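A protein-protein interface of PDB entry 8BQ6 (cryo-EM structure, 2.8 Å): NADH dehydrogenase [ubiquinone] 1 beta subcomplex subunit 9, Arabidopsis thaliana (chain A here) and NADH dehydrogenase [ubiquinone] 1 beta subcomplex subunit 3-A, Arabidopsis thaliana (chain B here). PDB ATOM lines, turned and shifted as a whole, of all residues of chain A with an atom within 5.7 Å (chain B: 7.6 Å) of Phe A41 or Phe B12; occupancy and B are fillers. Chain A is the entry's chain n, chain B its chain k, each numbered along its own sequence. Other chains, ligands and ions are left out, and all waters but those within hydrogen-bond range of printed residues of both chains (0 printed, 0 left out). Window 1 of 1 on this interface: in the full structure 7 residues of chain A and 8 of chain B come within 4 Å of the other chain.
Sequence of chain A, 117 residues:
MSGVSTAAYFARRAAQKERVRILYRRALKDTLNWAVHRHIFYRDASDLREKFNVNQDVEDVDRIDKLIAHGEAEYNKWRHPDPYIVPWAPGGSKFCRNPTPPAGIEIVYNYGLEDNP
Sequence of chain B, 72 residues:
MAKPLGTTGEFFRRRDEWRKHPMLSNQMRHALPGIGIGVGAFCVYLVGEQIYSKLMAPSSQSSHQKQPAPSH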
ATOM      1  N   LEU A  28      -5.861  -3.611  17.458  1.00  0.00           N
ATOM      2  CA  LEU A  28      -4.857  -4.211  16.585  1.00  0.00           C
ATOM      3  C   LEU A  28      -3.704  -3.253  16.328  1.00  0.00           C
ATOM      4  O   LEU A  28      -2.546  -3.676  16.242  1.00  0.00           O
ATOM      5  CB  LEU A  28      -5.491  -4.653  15.268  1.00  0.00           C
ATOM      6  CG  LEU A  28      -4.742  -5.735  14.492  1.00  0.00           C
ATOM      7  CD1 LEU A  28      -4.295  -6.847  15.417  1.00  0.00           C
ATOM      8  CD2 LEU A  28      -5.634  -6.282  13.403  1.00  0.00           C
ATOM      9  N   THR A  31      -1.550  -2.939  19.428  1.00  0.00           N
ATOM     10  CA  THR A  31      -0.693  -4.106  19.589  1.00  0.00           C
ATOM     11  C   THR A  31       0.656  -3.881  18.922  1.00  0.00           C
ATOM     12  O   THR A  31       1.691  -4.337  19.421  1.00  0.00           O
ATOM     13  CB  THR A  31      -1.382  -5.335  19.005  1.00  0.00           C
ATOM     14  OG1 THR A  31      -2.606  -5.567  19.708  1.00  0.00           O
ATOM     15  CG2 THR A  31      -0.498  -6.549  19.165  1.00  0.00           C
ATOM     16  N   LEU A  32       0.664  -3.186  17.785  1.00  0.00           N
ATOM     17  CA  LEU A  32       1.926  -2.901  17.118  1.00  0.00           C
ATOM     18  C   LEU A  32       2.734  -1.865  17.894  1.00  0.00           C
ATOM     19  O   LEU A  32       3.967  -1.839  17.803  1.00  0.00           O
ATOM     20  CB  LEU A  32       1.660  -2.447  15.683  1.00  0.00           C
ATOM     21  CG  LEU A  32       2.858  -2.262  14.754  1.00  0.00           C
ATOM     22  CD1 LEU A  32       3.890  -3.362  14.957  1.00  0.00           C
ATOM     23  CD2 LEU A  32       2.391  -2.239  13.318  1.00  0.00           C
ATOM     24  N   ALA A  35       4.575  -3.904  20.540  1.00  0.00           N
ATOM     25  CA  ALA A  35       5.466  -4.952  19.993  1.00  0.00           C
ATOM     26  C   ALA A  35       6.669  -4.364  19.253  1.00  0.00           C
ATOM     27  O   ALA A  35       7.735  -5.004  19.377  1.00  0.00           O
ATOM     28  CB  ALA A  35       4.656  -5.831  19.080  1.00  0.00           C
ATOM     29  N   HIS A  37       8.581  -4.631  16.908  1.00  0.00           N
ATOM     30  CA  HIS A  37       9.118  -5.514  15.884  1.00  0.00           C
ATOM     31  C   HIS A  37       8.014  -6.267  15.161  1.00  0.00           C
ATOM     32  O   HIS A  37       7.020  -6.684  15.764  1.00  0.00           O
ATOM     33  CB  HIS A  37      10.110  -6.499  16.494  1.00  0.00           C
ATOM     34  CG  HIS A  37      11.307  -5.837  17.091  1.00  0.00           C
ATOM     35  ND1 HIS A  37      11.788  -4.630  16.632  1.00  0.00           N
ATOM     36  CD2 HIS A  37      12.137  -6.217  18.089  1.00  0.00           C
ATOM     37  CE1 HIS A  37      12.851  -4.287  17.334  1.00  0.00           C
ATOM     38  NE2 HIS A  37      13.085  -5.233  18.224  1.00  0.00           N
ATOM     39  N   ARG A  38       8.208  -6.445  13.853  1.00  0.00           N
ATOM     40  CA  ARG A  38       7.198  -7.086  13.023  1.00  0.00           C
ATOM     41  C   ARG A  38       6.915  -8.505  13.492  1.00  0.00           C
ATOM     42  O   ARG A  38       5.756  -8.888  13.682  1.00  0.00           O
ATOM     43  CB  ARG A  38       7.652  -7.085  11.565  1.00  0.00           C
ATOM     44  CG  ARG A  38       7.986  -5.709  11.034  1.00  0.00           C
ATOM     45  CD  ARG A  38       6.788  -4.803  11.183  1.00  0.00           C
ATOM     46  NE  ARG A  38       5.719  -5.225  10.287  1.00  0.00           N
ATOM     47  CZ  ARG A  38       4.561  -4.597  10.146  1.00  0.00           C
ATOM     48  NH1 ARG A  38       4.273  -3.510  10.843  1.00  0.00           N
ATOM     49  NH2 ARG A  38       3.667  -5.076   9.287  1.00  0.00           N
ATOM     50  N   HIS A  39       7.968  -9.298  13.704  1.00  0.00           N
ATOM     51  CA  HIS A  39       7.744 -10.702  14.025  1.00  0.00           C
ATOM     52  C   HIS A  39       6.999 -10.867  15.344  1.00  0.00           C
ATOM     53  O   HIS A  39       6.129 -11.737  15.447  1.00  0.00           O
ATOM     54  CB  HIS A  39       9.065 -11.477  14.013  1.00  0.00           C
ATOM     55  CG  HIS A  39       9.996 -11.141  15.135  1.00  0.00           C
ATOM     56  ND1 HIS A  39      10.909 -10.112  15.063  1.00  0.00           N
ATOM     57  CD2 HIS A  39      10.131 -11.677  16.372  1.00  0.00           C
ATOM     58  CE1 HIS A  39      11.575 -10.036  16.201  1.00  0.00           C
ATOM     59  NE2 HIS A  39      11.125 -10.976  17.011  1.00  0.00           N
ATOM     60  N   ILE A  40       7.282  -9.994  16.320  1.00  0.00           N
ATOM     61  CA  ILE A  40       6.551 -10.035  17.623  1.00  0.00           C
ATOM     62  C   ILE A  40       5.099  -9.609  17.381  1.00  0.00           C
ATOM     63  O   ILE A  40       4.224 -10.062  18.136  1.00  0.00           O
ATOM     64  CB  ILE A  40       7.237  -9.167  18.701  1.00  0.00           C
ATOM     65  CG1 ILE A  40       8.761  -9.180  18.591  1.00  0.00           C
ATOM     66  CG2 ILE A  40       6.789  -9.581  20.093  1.00  0.00           C
ATOM     67  CD1 ILE A  40       9.460  -8.469  19.726  1.00  0.00           C
ATOM     68  N   PHE A  41       4.850  -8.792  16.351  1.00  0.00           N
ATOM     69  CA  PHE A  41       3.500  -8.332  16.055  1.00  0.00           C
ATOM     70  C   PHE A  41       2.652  -9.447  15.451  1.00  0.00           C
ATOM     71  O   PHE A  41       1.439  -9.502  15.680  1.00  0.00           O
ATOM     72  CB  PHE A  41       3.563  -7.110  15.137  1.00  0.00           C
ATOM     73  CG  PHE A  41       2.238  -6.696  14.574  1.00  0.00           C
ATOM     74  CD1 PHE A  41       1.192  -6.345  15.411  1.00  0.00           C
ATOM     75  CD2 PHE A  41       2.050  -6.617  13.207  1.00  0.00           C
ATOM     76  CE1 PHE A  41      -0.024  -5.956  14.892  1.00  0.00           C
ATOM     77  CE2 PHE A  41       0.838  -6.222  12.683  1.00  0.00           C
ATOM     78  CZ  PHE A  41      -0.200  -5.893  13.525  1.00  0.00           C
ATOM     79  N   TYR A  42       3.268 -10.354  14.685  1.00  0.00           N
ATOM     80  CA  TYR A  42       2.521 -11.481  14.129  1.00  0.00           C
ATOM     81  C   TYR A  42       1.926 -12.345  15.236  1.00  0.00           C
ATOM     82  O   TYR A  42       0.737 -12.678  15.214  1.00  0.00           O
ATOM     83  CB  TYR A  42       3.418 -12.337  13.231  1.00  0.00           C
ATOM     84  CG  TYR A  42       4.246 -11.584  12.218  1.00  0.00           C
ATOM     85  CD1 TYR A  42       3.801 -10.395  11.655  1.00  0.00           C
ATOM     86  CD2 TYR A  42       5.482 -12.069  11.827  1.00  0.00           C
ATOM     87  CE1 TYR A  42       4.570  -9.717  10.730  1.00  0.00           C
ATOM     88  CE2 TYR A  42       6.254 -11.399  10.913  1.00  0.00           C
ATOM     89  CZ  TYR A  42       5.798 -10.228  10.365  1.00  0.00           C
ATOM     90  OH  TYR A  42       6.587  -9.576   9.450  1.00  0.00           O
ATOM     91  N   ARG A  43       2.750 -12.719  16.219  1.00  0.00           N
ATOM     92  CA  ARG A  43       2.270 -13.569  17.304  1.00  0.00           C
ATOM     93  C   ARG A  43       1.205 -12.860  18.131  1.00  0.00           C
ATOM     94  O   ARG A  43       0.204 -13.469  18.523  1.00  0.00           O
ATOM     95  CB  ARG A  43       3.434 -13.991  18.197  1.00  0.00           C
ATOM     96  CG  ARG A  43       3.047 -14.900  19.347  1.00  0.00           C
ATOM     97  CD  ARG A  43       4.284 -15.312  20.116  1.00  0.00           C
ATOM     98  NE  ARG A  43       3.943 -16.205  21.215  1.00  0.00           N
ATOM     99  CZ  ARG A  43       4.831 -16.872  21.936  1.00  0.00           C
ATOM    100  NH1 ARG A  43       6.131 -16.709  21.753  1.00  0.00           N
ATOM    101  NH2 ARG A  43       4.405 -17.726  22.862  1.00  0.00           N
ATOM    102  N   ASP A  44       1.423 -11.571  18.390  1.00  0.00           N
ATOM    103  CA  ASP A  44       0.485 -10.807  19.255  1.00  0.00           C
ATOM    104  C   ASP A  44      -0.821 -10.495  18.507  1.00  0.00           C
ATOM    105  O   ASP A  44      -1.865 -10.435  19.183  1.00  0.00           O
ATOM    106  CB  ASP A  44       1.178  -9.566  19.818  1.00  0.00           C
ATOM    107  CG  ASP A  44       2.231  -9.887  20.867  1.00  0.00           C
ATOM    108  OD1 ASP A  44       2.231 -11.027  21.364  1.00  0.00           O
ATOM    109  OD2 ASP A  44       3.045  -8.992  21.174  1.00  0.00           O
ATOM    110  N   ALA A  45      -0.774 -10.304  17.183  1.00  0.00           N
ATOM    111  CA  ALA A  45      -1.993 -10.078  16.413  1.00  0.00           C
ATOM    112  C   ALA A  45      -2.846 -11.335  16.355  1.00  0.00           C
ATOM    113  O   ALA A  45      -4.076 -11.266  16.456  1.00  0.00           O
ATOM    114  CB  ALA A  45      -1.649  -9.598  15.004  1.00  0.00           C
ATOM    115  N   SER A  46      -2.210 -12.497  16.191  1.00  0.00           N
ATOM    116  CA  SER A  46      -2.961 -13.746  16.183  1.00  0.00           C
ATOM    117  C   SER A  46      -3.687 -13.953  17.506  1.00  0.00           C
ATOM    118  O   SER A  46      -4.850 -14.371  17.526  1.00  0.00           O
ATOM    119  CB  SER A  46      -2.026 -14.919  15.892  1.00  0.00           C
ATOM    120  OG  SER A  46      -2.762 -16.112  15.704  1.00  0.00           O
ATOM    121  N   PRO B   4       3.041 -15.876  13.459  1.00  0.00           N
ATOM    122  CA  PRO B   4       2.320 -15.907  12.177  1.00  0.00           C
ATOM    123  C   PRO B   4       1.516 -17.203  11.997  1.00  0.00           C
ATOM    124  O   PRO B   4       1.194 -17.533  10.867  1.00  0.00           O
ATOM    125  CB  PRO B   4       3.431 -15.811  11.119  1.00  0.00           C
ATOM    126  CG  PRO B   4       4.616 -16.458  11.785  1.00  0.00           C
ATOM    127  CD  PRO B   4       4.478 -16.085  13.247  1.00  0.00           C
ATOM    128  N   GLY B   6      -1.712 -18.031  13.266  1.00  0.00           N
ATOM    129  CA  GLY B   6      -3.112 -17.730  12.907  1.00  0.00           C
ATOM    130  C   GLY B   6      -3.228 -16.919  11.628  1.00  0.00           C
ATOM    131  O   GLY B   6      -2.215 -16.331  11.202  1.00  0.00           O
ATOM    132  N   THR B   7      -4.427 -16.878  11.042  1.00  0.00           N
ATOM    133  CA  THR B   7      -4.639 -16.154   9.758  1.00  0.00           C
ATOM    134  C   THR B   7      -4.242 -14.679   9.910  1.00  0.00           C
ATOM    135  O   THR B   7      -3.769 -14.107   8.910  1.00  0.00           O
ATOM    136  CB  THR B   7      -6.079 -16.325   9.261  1.00  0.00           C
ATOM    137  OG1 THR B   7      -6.968 -15.681  10.176  1.00  0.00           O
ATOM    138  CG2 THR B   7      -6.464 -17.780   9.110  1.00  0.00           C
ATOM    139  N   THR B   8      -4.419 -14.096  11.102  1.00  0.00           N
ATOM    140  CA  THR B   8      -3.995 -12.718  11.310  1.00  0.00           C
ATOM    141  C   THR B   8      -2.485 -12.592  11.161  1.00  0.00           C
ATOM    142  O   THR B   8      -1.991 -11.724  10.432  1.00  0.00           O
ATOM    143  CB  THR B   8      -4.436 -12.237  12.692  1.00  0.00           C
ATOM    144  OG1 THR B   8      -5.835 -12.485  12.854  1.00  0.00           O
ATOM    145  CG2 THR B   8      -4.199 -10.749  12.824  1.00  0.00           C
ATOM    146  N   GLY B   9      -1.733 -13.465  11.836  1.00  0.00           N
ATOM    147  CA  GLY B   9      -0.286 -13.425  11.728  1.00  0.00           C
ATOM    148  C   GLY B   9       0.223 -13.779  10.345  1.00  0.00           C
ATOM    149  O   GLY B   9       1.198 -13.192   9.871  1.00  0.00           O
ATOM    150  N   GLU B  10      -0.427 -14.738   9.679  1.00  0.00           N
ATOM    151  CA  GLU B  10       0.036 -15.179   8.366  1.00  0.00           C
ATOM    152  C   GLU B  10      -0.118 -14.076   7.330  1.00  0.00           C
ATOM    153  O   GLU B  10       0.691 -13.963   6.402  1.00  0.00           O
ATOM    154  CB  GLU B  10      -0.729 -16.431   7.934  1.00  0.00           C
ATOM    155  CG  GLU B  10      -0.408 -16.921   6.529  1.00  0.00           C
ATOM    156  CD  GLU B  10       1.080 -17.108   6.298  1.00  0.00           C
ATOM    157  OE1 GLU B  10       1.743 -17.713   7.168  1.00  0.00           O
ATOM    158  OE2 GLU B  10       1.581 -16.664   5.242  1.00  0.00           O
ATOM    159  N   PHE B  11      -1.163 -13.260   7.470  1.00  0.00           N
ATOM    160  CA  PHE B  11      -1.358 -12.136   6.563  1.00  0.00           C
ATOM    161  C   PHE B  11      -0.192 -11.161   6.634  1.00  0.00           C
ATOM    162  O   PHE B  11       0.392 -10.800   5.605  1.00  0.00           O
ATOM    163  CB  PHE B  11      -2.657 -11.417   6.916  1.00  0.00           C
ATOM    164  CG  PHE B  11      -3.069 -10.380   5.919  1.00  0.00           C
ATOM    165  CD1 PHE B  11      -2.456 -10.290   4.683  1.00  0.00           C
ATOM    166  CD2 PHE B  11      -4.030  -9.448   6.250  1.00  0.00           C
ATOM    167  CE1 PHE B  11      -2.830  -9.321   3.783  1.00  0.00           C
ATOM    168  CE2 PHE B  11      -4.404  -8.476   5.353  1.00  0.00           C
ATOM    169  CZ  PHE B  11      -3.804  -8.411   4.119  1.00  0.00           C
ATOM    170  N   PHE B  12       0.160 -10.726   7.842  1.00  0.00           N
ATOM    171  CA  PHE B  12       1.117  -9.638   7.979  1.00  0.00           C
ATOM    172  C   PHE B  12       2.526 -10.071   7.595  1.00  0.00           C
ATOM    173  O   PHE B  12       3.278  -9.272   7.026  1.00  0.00           O
ATOM    174  CB  PHE B  12       1.046  -9.087   9.401  1.00  0.00           C
ATOM    175  CG  PHE B  12      -0.209  -8.302   9.665  1.00  0.00           C
ATOM    176  CD1 PHE B  12      -0.611  -7.312   8.785  1.00  0.00           C
ATOM    177  CD2 PHE B  12      -1.011  -8.583  10.757  1.00  0.00           C
ATOM    178  CE1 PHE B  12      -1.767  -6.593   9.005  1.00  0.00           C
ATOM    179  CE2 PHE B  12      -2.171  -7.870  10.981  1.00  0.00           C
ATOM    180  CZ  PHE B  12      -2.551  -6.874  10.102  1.00  0.00           C
ATOM    181  N   ARG B  13       2.896 -11.325   7.864  1.00  0.00           N
ATOM    182  CA  ARG B  13       4.174 -11.818   7.359  1.00  0.00           C
ATOM    183  C   ARG B  13       4.181 -11.884   5.839  1.00  0.00           C
ATOM    184  O   ARG B  13       5.214 -11.633   5.208  1.00  0.00           O
ATOM    185  CB  ARG B  13       4.503 -13.188   7.937  1.00  0.00           C
ATOM    186  CG  ARG B  13       5.989 -13.371   8.141  1.00  0.00           C
ATOM    187  CD  ARG B  13       6.394 -14.819   8.018  1.00  0.00           C
ATOM    188  NE  ARG B  13       6.978 -15.121   6.717  1.00  0.00           N
ATOM    189  CZ  ARG B  13       6.598 -16.127   5.942  1.00  0.00           C
ATOM    190  NH1 ARG B  13       5.615 -16.940   6.299  1.00  0.00           N
ATOM    191  NH2 ARG B  13       7.221 -16.327   4.785  1.00  0.00           N
ATOM    192  N   ARG B  14       3.051 -12.249   5.237  1.00  0.00           N
ATOM    193  CA  ARG B  14       2.978 -12.265   3.783  1.00  0.00           C
ATOM    194  C   ARG B  14       3.167 -10.868   3.209  1.00  0.00           C
ATOM    195  O   ARG B  14       3.823 -10.696   2.177  1.00  0.00           O
ATOM    196  CB  ARG B  14       1.647 -12.854   3.327  1.00  0.00           C
ATOM    197  CG  ARG B  14       1.760 -13.621   2.035  1.00  0.00           C
ATOM    198  CD  ARG B  14       2.146 -15.070   2.289  1.00  0.00           C
ATOM    199  NE  ARG B  14       1.099 -15.800   2.995  1.00  0.00           N
ATOM    200  CZ  ARG B  14      -0.101 -16.065   2.496  1.00  0.00           C
ATOM    201  NH1 ARG B  14      -0.451 -15.667   1.283  1.00  0.00           N
ATOM    202  NH2 ARG B  14      -0.974 -16.750   3.230  1.00  0.00           N
ATOM    203  N   ARG B  15       2.597  -9.855   3.862  1.00  0.00           N
ATOM    204  CA  ARG B  15       2.775  -8.482   3.405  1.00  0.00           C
ATOM    205  C   ARG B  15       4.155  -7.927   3.728  1.00  0.00           C
ATOM    206  O   ARG B  15       4.585  -6.963   3.087  1.00  0.00           O
ATOM    207  CB  ARG B  15       1.712  -7.585   4.022  1.00  0.00           C
ATOM    208  CG  ARG B  15       0.303  -7.991   3.681  1.00  0.00           C
ATOM    209  CD  ARG B  15       0.009  -7.811   2.197  1.00  0.00           C
ATOM    210  NE  ARG B  15       0.567  -6.575   1.660  1.00  0.00           N
ATOM    211  CZ  ARG B  15       0.935  -6.405   0.398  1.00  0.00           C
ATOM    212  NH1 ARG B  15       0.749  -7.350  -0.510  1.00  0.00           N
ATOM    213  NH2 ARG B  15       1.496  -5.256   0.033  1.00  0.00           N
ATOM    214  N   ASP B  16       4.844  -8.494   4.718  1.00  0.00           N
ATOM    215  CA  ASP B  16       6.178  -8.062   5.108  1.00  0.00           C
ATOM    216  C   ASP B  16       7.255  -8.745   4.299  1.00  0.00           C
ATOM    217  O   ASP B  16       8.431  -8.722   4.683  1.00  0.00           O
ATOM    218  CB  ASP B  16       6.401  -8.331   6.591  1.00  0.00           C
ATOM    219  CG  ASP B  16       5.796  -7.269   7.458  1.00  0.00           C
ATOM    220  OD1 ASP B  16       5.978  -6.078   7.134  1.00  0.00           O
ATOM    221  OD2 ASP B  16       5.125  -7.619   8.448  1.00  0.00           O
ATOM    222  N   GLU B  17       6.871  -9.363   3.191  1.00  0.00           N
ATOM    223  CA  GLU B  17       7.798 -10.213   2.464  1.00  0.00           C
ATOM    224  C   GLU B  17       8.812  -9.389   1.680  1.00  0.00           C
ATOM    225  O   GLU B  17       9.842  -9.925   1.257  1.00  0.00           O
ATOM    226  CB  GLU B  17       6.974 -11.195   1.613  1.00  0.00           C
ATOM    227  CG  GLU B  17       6.165 -12.216   2.385  1.00  0.00           C
ATOM    228  CD  GLU B  17       5.349 -13.075   1.519  1.00  0.00           C
ATOM    229  OE1 GLU B  17       5.266 -12.752   0.324  1.00  0.00           O
ATOM    230  OE2 GLU B  17       4.746 -14.044   2.052  1.00  0.00           O
ATOM    231  N   ARG B  19      10.427  -7.067   3.267  1.00  0.00           N
ATOM    232  CA  ARG B  19      11.423  -6.721   4.280  1.00  0.00           C
ATOM    233  C   ARG B  19      12.626  -7.652   4.272  1.00  0.00           C
ATOM    234  O   ARG B  19      13.560  -7.435   5.052  1.00  0.00           O
ATOM    235  CB  ARG B  19      10.785  -6.707   5.669  1.00  0.00           C
ATOM    236  CG  ARG B  19      10.056  -5.413   5.971  1.00  0.00           C
ATOM    237  CD  ARG B  19       9.258  -5.493   7.248  1.00  0.00           C
ATOM    238  NE  ARG B  19       7.972  -4.823   7.107  1.00  0.00           N
ATOM    239  CZ  ARG B  19       7.770  -3.537   7.357  1.00  0.00           C
ATOM    240  NH1 ARG B  19       8.759  -2.742   7.732  1.00  0.00           N
ATOM    241  NH2 ARG B  19       6.547  -3.036   7.224  1.00  0.00           N
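Arg A38 touches Arg B19.
CE2 of Phe A41 touches CD2 of Phe B12, at 3.6 Å.
Pro B4 touches Tyr A42 (N to CB, 3.6 Å).
Gly B9 touches Tyr A42.
CE1 of Tyr A42 touches C of Phe B12 (3.8 Å).
CE2 of Tyr A42 touches CG of Arg B13, at 3.4 Å.
Ala A45 touches Thr B8 (CB to CG2, 3.5 Å).
Of chain B, only Phe B12 comes within 4 Å of Phe A41.
Printed residues of chain B within 4 Å of Tyr A42: Pro B4, Gly B9, Phe B12, Arg B13 and Asp B16.
Printed residues of chain B within 4 Å of Ser A46: Gly B6 (3.3 Å).
Of the printed residues of chain A, Gly B6 touches Ser A46 (3.3 Å).
Printed residues of chain A within 4 Å of Thr B8: Ala A45 (3.5 Å).
Phe B12 touches two residues of chain A.
Of the printed residues of chain A, Arg B13 touches Tyr A42.
The nearest printed residue of chain A that does not touch Pro B4 is Arg A43 (4.2 Å).
OH of Tyr A42 is in hydrogen-bond range of OD2 of Asp B16 (2.6 Å).
NH2 of Arg A38 lies within salt-bridge range of OD2 of Asp B16 (3.0 Å).
OG of Ser A46 lies close to N of Gly B6, at 3.3 Å.
The backbone carbonyl oxygen of Pro B4 sits at hydrogen-bond distance from the backbone NH of Glu B10.
The side-chain carboxylate (OD1) of Asp B16 is in salt-bridge range of the guanidinium group (NH2) of Arg B19, 3.1 Å away.
Of the 14 printed residues of chain B, 8 touch a printed residue of chain A.
Printed residues of chain B that touch a printed residue of chain A: Pro B4, Gly B6, Thr B8, Gly B9, Phe B12, Arg B13, Asp B16 and Arg B19.
Of the 14 printed residues of chain A, 5 touch a printed residue of chain B.
Hydrophobic or aromatic side chains of chain A within 4 Å of the printed part of chain B: Phe A41, Tyr A42 and Ala A45.
Among the printed residues, 10 pairs touch across the chains.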
